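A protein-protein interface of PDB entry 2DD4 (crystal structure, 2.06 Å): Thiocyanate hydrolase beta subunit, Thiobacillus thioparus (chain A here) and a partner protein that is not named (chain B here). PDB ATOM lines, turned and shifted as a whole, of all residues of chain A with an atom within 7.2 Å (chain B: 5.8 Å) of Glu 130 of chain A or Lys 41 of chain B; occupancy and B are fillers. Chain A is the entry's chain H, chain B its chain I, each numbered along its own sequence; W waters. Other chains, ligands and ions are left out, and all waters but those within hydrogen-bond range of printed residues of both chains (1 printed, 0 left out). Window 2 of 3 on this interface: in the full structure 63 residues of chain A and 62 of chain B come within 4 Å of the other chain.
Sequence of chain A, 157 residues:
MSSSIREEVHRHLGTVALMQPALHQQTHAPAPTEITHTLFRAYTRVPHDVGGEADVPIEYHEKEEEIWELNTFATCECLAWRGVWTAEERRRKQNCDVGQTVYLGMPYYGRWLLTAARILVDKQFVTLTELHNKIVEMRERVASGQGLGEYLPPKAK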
ATOM      1  N   LEU A 120      24.402 -24.757  20.934  1.00  0.00           N
ATOM      2  CA  LEU A 120      24.023 -23.403  21.345  1.00  0.00           C
ATOM      3  C   LEU A 120      25.159 -22.423  21.052  1.00  0.00           C
ATOM      4  O   LEU A 120      24.928 -21.311  20.578  1.00  0.00           O
ATOM      5  CB  LEU A 120      23.694 -23.351  22.843  1.00  0.00           C
ATOM      6  CG  LEU A 120      22.603 -24.262  23.416  1.00  0.00           C
ATOM      7  CD1 LEU A 120      22.326 -23.853  24.863  1.00  0.00           C
ATOM      8  CD2 LEU A 120      21.338 -24.157  22.591  1.00  0.00           C
ATOM      9  N   GLN A 124      25.933 -19.753  17.663  1.00  0.00           N
ATOM     10  CA  GLN A 124      25.872 -18.458  18.331  1.00  0.00           C
ATOM     11  C   GLN A 124      24.542 -18.058  18.975  1.00  0.00           C
ATOM     12  O   GLN A 124      24.187 -16.879  18.984  1.00  0.00           O
ATOM     13  CB  GLN A 124      26.322 -17.366  17.351  1.00  0.00           C
ATOM     14  CG  GLN A 124      27.760 -17.538  16.868  1.00  0.00           C
ATOM     15  CD  GLN A 124      28.138 -16.558  15.767  1.00  0.00           C
ATOM     16  OE1 GLN A 124      27.466 -16.475  14.741  1.00  0.00           O
ATOM     17  NE2 GLN A 124      29.219 -15.819  15.975  1.00  0.00           N
ATOM     18  N   PHE A 125      23.802 -19.022  19.513  1.00  0.00           N
ATOM     19  CA  PHE A 125      22.551 -18.691  20.182  1.00  0.00           C
ATOM     20  C   PHE A 125      22.908 -18.197  21.580  1.00  0.00           C
ATOM     21  O   PHE A 125      22.112 -17.540  22.246  1.00  0.00           O
ATOM     22  CB  PHE A 125      21.624 -19.901  20.233  1.00  0.00           C
ATOM     23  CG  PHE A 125      21.031 -20.250  18.896  1.00  0.00           C
ATOM     24  CD1 PHE A 125      20.264 -19.316  18.201  1.00  0.00           C
ATOM     25  CD2 PHE A 125      21.259 -21.493  18.319  1.00  0.00           C
ATOM     26  CE1 PHE A 125      19.735 -19.617  16.947  1.00  0.00           C
ATOM     27  CE2 PHE A 125      20.733 -21.804  17.065  1.00  0.00           C
ATOM     28  CZ  PHE A 125      19.970 -20.863  16.379  1.00  0.00           C
ATOM     29  N   VAL A 126      24.127 -18.532  22.004  1.00  0.00           N
ATOM     30  CA  VAL A 126      24.683 -18.104  23.283  1.00  0.00           C
ATOM     31  C   VAL A 126      26.192 -18.000  23.064  1.00  0.00           C
ATOM     32  O   VAL A 126      26.765 -18.753  22.270  1.00  0.00           O
ATOM     33  CB  VAL A 126      24.439 -19.126  24.446  1.00  0.00           C
ATOM     34  CG1 VAL A 126      22.953 -19.466  24.562  1.00  0.00           C
ATOM     35  CG2 VAL A 126      25.278 -20.379  24.236  1.00  0.00           C
ATOM     36  N   THR A 127      26.835 -17.057  23.743  1.00  0.00           N
ATOM     37  CA  THR A 127      28.280 -16.931  23.622  1.00  0.00           C
ATOM     38  C   THR A 127      28.851 -17.975  24.577  1.00  0.00           C
ATOM     39  O   THR A 127      28.155 -18.439  25.485  1.00  0.00           O
ATOM     40  CB  THR A 127      28.774 -15.545  24.069  1.00  0.00           C
ATOM     41  OG1 THR A 127      28.428 -15.339  25.445  1.00  0.00           O
ATOM     42  CG2 THR A 127      28.148 -14.447  23.210  1.00  0.00           C
ATOM     43  N   LEU A 128      30.105 -18.361  24.376  1.00  0.00           N
ATOM     44  CA  LEU A 128      30.711 -19.331  25.274  1.00  0.00           C
ATOM     45  C   LEU A 128      30.748 -18.678  26.655  1.00  0.00           C
ATOM     46  O   LEU A 128      30.646 -19.347  27.679  1.00  0.00           O
ATOM     47  CB  LEU A 128      32.134 -19.674  24.825  1.00  0.00           C
ATOM     48  CG  LEU A 128      32.841 -20.740  25.671  1.00  0.00           C
ATOM     49  CD1 LEU A 128      32.059 -22.041  25.615  1.00  0.00           C
ATOM     50  CD2 LEU A 128      34.260 -20.951  25.153  1.00  0.00           C
ATOM     51  N   THR A 129      30.892 -17.357  26.668  1.00  0.00           N
ATOM     52  CA  THR A 129      30.936 -16.601  27.916  1.00  0.00           C
ATOM     53  C   THR A 129      29.631 -16.790  28.694  1.00  0.00           C
ATOM     54  O   THR A 129      29.650 -16.997  29.906  1.00  0.00           O
ATOM     55  CB  THR A 129      31.156 -15.102  27.634  1.00  0.00           C
ATOM     56  OG1 THR A 129      32.407 -14.931  26.954  1.00  0.00           O
ATOM     57  CG2 THR A 129      31.166 -14.297  28.936  1.00  0.00           C
ATOM     58  N   GLU A 130      28.499 -16.726  27.998  1.00  0.00           N
ATOM     59  CA  GLU A 130      27.215 -16.915  28.662  1.00  0.00           C
ATOM     60  C   GLU A 130      27.119 -18.326  29.250  1.00  0.00           C
ATOM     61  O   GLU A 130      26.597 -18.511  30.352  1.00  0.00           O
ATOM     62  CB  GLU A 130      26.061 -16.665  27.684  1.00  0.00           C
ATOM     63  CG  GLU A 130      25.885 -15.196  27.289  1.00  0.00           C
ATOM     64  CD  GLU A 130      24.791 -14.994  26.250  1.00  0.00           C
ATOM     65  OE1 GLU A 130      24.866 -15.619  25.171  1.00  0.00           O
ATOM     66  OE2 GLU A 130      23.856 -14.205  26.506  1.00  0.00           O
ATOM     67  N   LEU A 131      27.631 -19.320  28.526  1.00  0.00           N
ATOM     68  CA  LEU A 131      27.594 -20.700  29.009  1.00  0.00           C
ATOM     69  C   LEU A 131      28.480 -20.845  30.245  1.00  0.00           C
ATOM     70  O   LEU A 131      28.041 -21.368  31.269  1.00  0.00           O
ATOM     71  CB  LEU A 131      28.054 -21.673  27.915  1.00  0.00           C
ATOM     72  CG  LEU A 131      28.146 -23.158  28.311  1.00  0.00           C
ATOM     73  CD1 LEU A 131      26.819 -23.638  28.871  1.00  0.00           C
ATOM     74  CD2 LEU A 131      28.535 -23.987  27.097  1.00  0.00           C
ATOM     75  N   HIS A 132      29.728 -20.388  30.148  1.00  0.00           N
ATOM     76  CA  HIS A 132      30.652 -20.454  31.279  1.00  0.00           C
ATOM     77  C   HIS A 132      30.050 -19.742  32.490  1.00  0.00           C
ATOM     78  O   HIS A 132      30.114 -20.246  33.615  1.00  0.00           O
ATOM     79  CB  HIS A 132      31.992 -19.788  30.934  1.00  0.00           C
ATOM     80  CG  HIS A 132      32.852 -20.587  30.003  1.00  0.00           C
ATOM     81  ND1 HIS A 132      34.073 -20.133  29.549  1.00  0.00           N
ATOM     82  CD2 HIS A 132      32.676 -21.813  29.451  1.00  0.00           C
ATOM     83  CE1 HIS A 132      34.613 -21.045  28.759  1.00  0.00           C
ATOM     84  NE2 HIS A 132      33.786 -22.073  28.683  1.00  0.00           N
ATOM     85  N   ASN A 133      29.464 -18.571  32.256  1.00  0.00           N
ATOM     86  CA  ASN A 133      28.867 -17.794  33.340  1.00  0.00           C
ATOM     87  C   ASN A 133      27.669 -18.483  33.981  1.00  0.00           C
ATOM     88  O   ASN A 133      27.489 -18.409  35.195  1.00  0.00           O
ATOM     89  CB  ASN A 133      28.463 -16.401  32.846  1.00  0.00           C
ATOM     90  CG  ASN A 133      29.664 -15.500  32.606  1.00  0.00           C
ATOM     91  OD1 ASN A 133      30.790 -15.816  33.012  1.00  0.00           O
ATOM     92  ND2 ASN A 133      29.430 -14.366  31.955  1.00  0.00           N
ATOM     93  N   LYS A 134      26.856 -19.148  33.165  1.00  0.00           N
ATOM     94  CA  LYS A 134      25.684 -19.858  33.664  1.00  0.00           C
ATOM     95  C   LYS A 134      26.125 -21.040  34.532  1.00  0.00           C
ATOM     96  O   LYS A 134      25.480 -21.361  35.529  1.00  0.00           O
ATOM     97  CB  LYS A 134      24.822 -20.344  32.489  1.00  0.00           C
ATOM     98  CG  LYS A 134      23.685 -21.293  32.869  1.00  0.00           C
ATOM     99  CD  LYS A 134      22.622 -20.644  33.753  1.00  0.00           C
ATOM    100  CE  LYS A 134      21.728 -19.684  32.978  1.00  0.00           C
ATOM    101  NZ  LYS A 134      20.566 -19.215  33.799  1.00  0.00           N
ATOM    102  N   ILE A 135      27.224 -21.687  34.153  1.00  0.00           N
ATOM    103  CA  ILE A 135      27.739 -22.818  34.924  1.00  0.00           C
ATOM    104  C   ILE A 135      28.269 -22.337  36.278  1.00  0.00           C
ATOM    105  O   ILE A 135      28.054 -22.987  37.301  1.00  0.00           O
ATOM    106  CB  ILE A 135      28.853 -23.557  34.145  1.00  0.00           C
ATOM    107  CG1 ILE A 135      28.232 -24.265  32.929  1.00  0.00           C
ATOM    108  CG2 ILE A 135      29.559 -24.566  35.052  1.00  0.00           C
ATOM    109  CD1 ILE A 135      29.239 -24.820  31.931  1.00  0.00           C
ATOM    110  N   VAL A 136      28.951 -21.196  36.286  1.00  0.00           N
ATOM    111  CA  VAL A 136      29.480 -20.638  37.530  1.00  0.00           C
ATOM    112  C   VAL A 136      28.330 -20.321  38.488  1.00  0.00           C
ATOM    113  O   VAL A 136      28.368 -20.677  39.664  1.00  0.00           O
ATOM    114  CB  VAL A 136      30.273 -19.332  37.282  1.00  0.00           C
ATOM    115  CG1 VAL A 136      30.649 -18.684  38.613  1.00  0.00           C
ATOM    116  CG2 VAL A 136      31.527 -19.632  36.475  1.00  0.00           C
ATOM    117  N   GLU B  36      18.170 -23.877  30.985  1.00  0.00           N
ATOM    118  CA  GLU B  36      17.835 -22.489  31.302  1.00  0.00           C
ATOM    119  C   GLU B  36      18.260 -21.537  30.189  1.00  0.00           C
ATOM    120  O   GLU B  36      17.515 -20.627  29.832  1.00  0.00           O
ATOM    121  CB  GLU B  36      18.459 -22.058  32.640  1.00  0.00           C
ATOM    122  CG  GLU B  36      17.768 -22.685  33.853  1.00  0.00           C
ATOM    123  CD  GLU B  36      18.178 -22.064  35.182  1.00  0.00           C
ATOM    124  OE1 GLU B  36      17.732 -22.579  36.230  1.00  0.00           O
ATOM    125  OE2 GLU B  36      18.933 -21.067  35.185  1.00  0.00           O
ATOM    126  N   LEU B  37      19.449 -21.751  29.633  1.00  0.00           N
ATOM    127  CA  LEU B  37      19.937 -20.899  28.554  1.00  0.00           C
ATOM    128  C   LEU B  37      19.054 -21.006  27.309  1.00  0.00           C
ATOM    129  O   LEU B  37      18.719 -19.993  26.683  1.00  0.00           O
ATOM    130  CB  LEU B  37      21.389 -21.261  28.206  1.00  0.00           C
ATOM    131  CG  LEU B  37      22.433 -20.784  29.228  1.00  0.00           C
ATOM    132  CD1 LEU B  37      23.798 -21.404  28.927  1.00  0.00           C
ATOM    133  CD2 LEU B  37      22.507 -19.265  29.192  1.00  0.00           C
ATOM    134  N   ALA B  38      18.673 -22.228  26.949  1.00  0.00           N
ATOM    135  CA  ALA B  38      17.834 -22.438  25.773  1.00  0.00           C
ATOM    136  C   ALA B  38      16.489 -21.726  25.930  1.00  0.00           C
ATOM    137  O   ALA B  38      15.981 -21.119  24.986  1.00  0.00           O
ATOM    138  CB  ALA B  38      17.611 -23.936  25.543  1.00  0.00           C
ATOM    139  N   ILE B  39      15.918 -21.808  27.126  1.00  0.00           N
ATOM    140  CA  ILE B  39      14.633 -21.179  27.399  1.00  0.00           C
ATOM    141  C   ILE B  39      14.769 -19.657  27.437  1.00  0.00           C
ATOM    142  O   ILE B  39      13.932 -18.944  26.891  1.00  0.00           O
ATOM    143  CB  ILE B  39      14.045 -21.703  28.732  1.00  0.00           C
ATOM    144  CG1 ILE B  39      13.690 -23.189  28.577  1.00  0.00           C
ATOM    145  CG2 ILE B  39      12.817 -20.885  29.129  1.00  0.00           C
ATOM    146  CD1 ILE B  39      13.178 -23.853  29.840  1.00  0.00           C
ATOM    147  N   GLU B  40      15.826 -19.169  28.078  1.00  0.00           N
ATOM    148  CA  GLU B  40      16.075 -17.733  28.170  1.00  0.00           C
ATOM    149  C   GLU B  40      16.252 -17.125  26.783  1.00  0.00           C
ATOM    150  O   GLU B  40      15.821 -16.000  26.535  1.00  0.00           O
ATOM    151  CB  GLU B  40      17.327 -17.461  29.022  1.00  0.00           C
ATOM    152  CG  GLU B  40      17.121 -17.729  30.512  1.00  0.00           C
ATOM    153  CD  GLU B  40      18.411 -17.686  31.321  1.00  0.00           C
ATOM    154  OE1 GLU B  40      18.342 -17.901  32.549  1.00  0.00           O
ATOM    155  OE2 GLU B  40      19.492 -17.445  30.737  1.00  0.00           O
ATOM    156  N   LYS B  41      16.882 -17.872  25.878  1.00  0.00           N
ATOM    157  CA  LYS B  41      17.102 -17.391  24.517  1.00  0.00           C
ATOM    158  C   LYS B  41      15.913 -17.673  23.601  1.00  0.00           C
ATOM    159  O   LYS B  41      15.928 -17.310  22.426  1.00  0.00           O
ATOM    160  CB  LYS B  41      18.360 -18.029  23.928  1.00  0.00           C
ATOM    161  CG  LYS B  41      19.638 -17.649  24.652  1.00  0.00           C
ATOM    162  CD  LYS B  41      19.897 -16.150  24.579  1.00  0.00           C
ATOM    163  CE  LYS B  41      21.218 -15.806  25.251  1.00  0.00           C
ATOM    164  NZ  LYS B  41      21.480 -14.350  25.250  1.00  0.00           N
ATOM    165  N   GLY B  42      14.893 -18.331  24.138  1.00  0.00           N
ATOM    166  CA  GLY B  42      13.709 -18.631  23.352  1.00  0.00           C
ATOM    167  C   GLY B  42      13.877 -19.681  22.269  1.00  0.00           C
ATOM    168  O   GLY B  42      13.156 -19.657  21.270  1.00  0.00           O
ATOM    169  N   LEU B  43      14.820 -20.601  22.450  1.00  0.00           N
ATOM    170  CA  LEU B  43      15.046 -21.659  21.465  1.00  0.00           C
ATOM    171  C   LEU B  43      13.872 -22.638  21.527  1.00  0.00           C
ATOM    172  O   LEU B  43      13.382 -23.100  20.497  1.00  0.00           O
ATOM    173  CB  LEU B  43      16.382 -22.349  21.742  1.00  0.00           C
ATOM    174  CG  LEU B  43      17.542 -21.343  21.755  1.00  0.00           C
ATOM    175  CD1 LEU B  43      18.863 -22.081  21.894  1.00  0.00           C
ATOM    176  CD2 LEU B  43      17.531 -20.515  20.467  1.00  0.00           C
HETATM  177  O   HOH W   1      24.125 -14.234  23.109  1.00  0.00           O
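The side-chain amino group (NZ) of Lys 41 of chain B lies within salt-bridge range of the side-chain carboxylate (OE2) of Glu 130 of chain A, 2.7 Å away. The side-chain amino group (NZ) of Lys 134 of chain A lies within salt-bridge range of the side-chain carboxylate (OE2) of Glu 36 of chain B (2.8 Å). The side-chain amino group (NZ) of Lys 134 of chain A is in salt-bridge range of the side-chain carboxylate (OE1) of Glu 40 of chain B (2.9 Å).
O of Leu 120 of chain A is in hydrogen-bond range of N of Phe 125 of chain A (2.8 Å). O of Leu 120 of chain A lies within hydrogen-bond range of N of Val 126 of chain A. The backbone NH (N) of Thr 127 of chain A lies within hydrogen-bond range of the side-chain carboxylate (OE1) of Glu 130 of chain A (2.8 Å). O of Ala 38 of chain B lies within hydrogen-bond range of N of Leu 43 of chain B (2.8 Å).
Leu 43 of chain B touches Leu 120 of chain A. Lys 41 of chain B touches Phe 125 of chain A. Leu 43 of chain B touches Phe 125 of chain A (CD2 to CD1, 3.7 Å). Lys 41 of chain B touches Val 126 of chain A. Leu 131 of chain A touches Leu 37 of chain B. Leu 37 of chain B touches Lys 134 of chain A.
Glu 130 of chain A touches just one residue of chain B: Lys 41 (2.7 Å). Printed residues of chain B within 4 Å of Lys 134 of chain A: Glu 36, Leu 37 and Glu 40. Of the printed residues of chain B, Phe 125 of chain A touches Lys 41 and Leu 43. Of the printed residues of chain A, Glu 40 of chain B touches Lys 134 (2.9 Å). Thr 129 of chain A touches none of the printed residues of chain B. The nearest residue of chain B that does not touch Glu 130 of chain A is Leu 37 of chain B (4.3 Å). The nearest residue of chain A that does not touch Lys 41 of chain B is Thr 127 of chain A (5.9 Å).
Of the 14 printed residues of chain A, 6 touch a printed residue of chain B. Along chain A the printed residues that touch a printed residue of chain B span positions 120 to 134. Along chain B the printed residues that touch a printed residue of chain A span positions 36 to 43. Among the printed residues, Asp or Glu carboxylates within 4 Å of a Lys or Arg side-chain nitrogen of the other chain: Glu 130 of chain A with Lys 41 of chain B, Lys 134 of chain A with Glu 36 of chain B and Lys 134 of chain A with Glu 40 of chain B.
Water W1 lies within hydrogen-bond range of OE1 of Glu 130 of chain A and NZ of Lys 41 of chain B.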
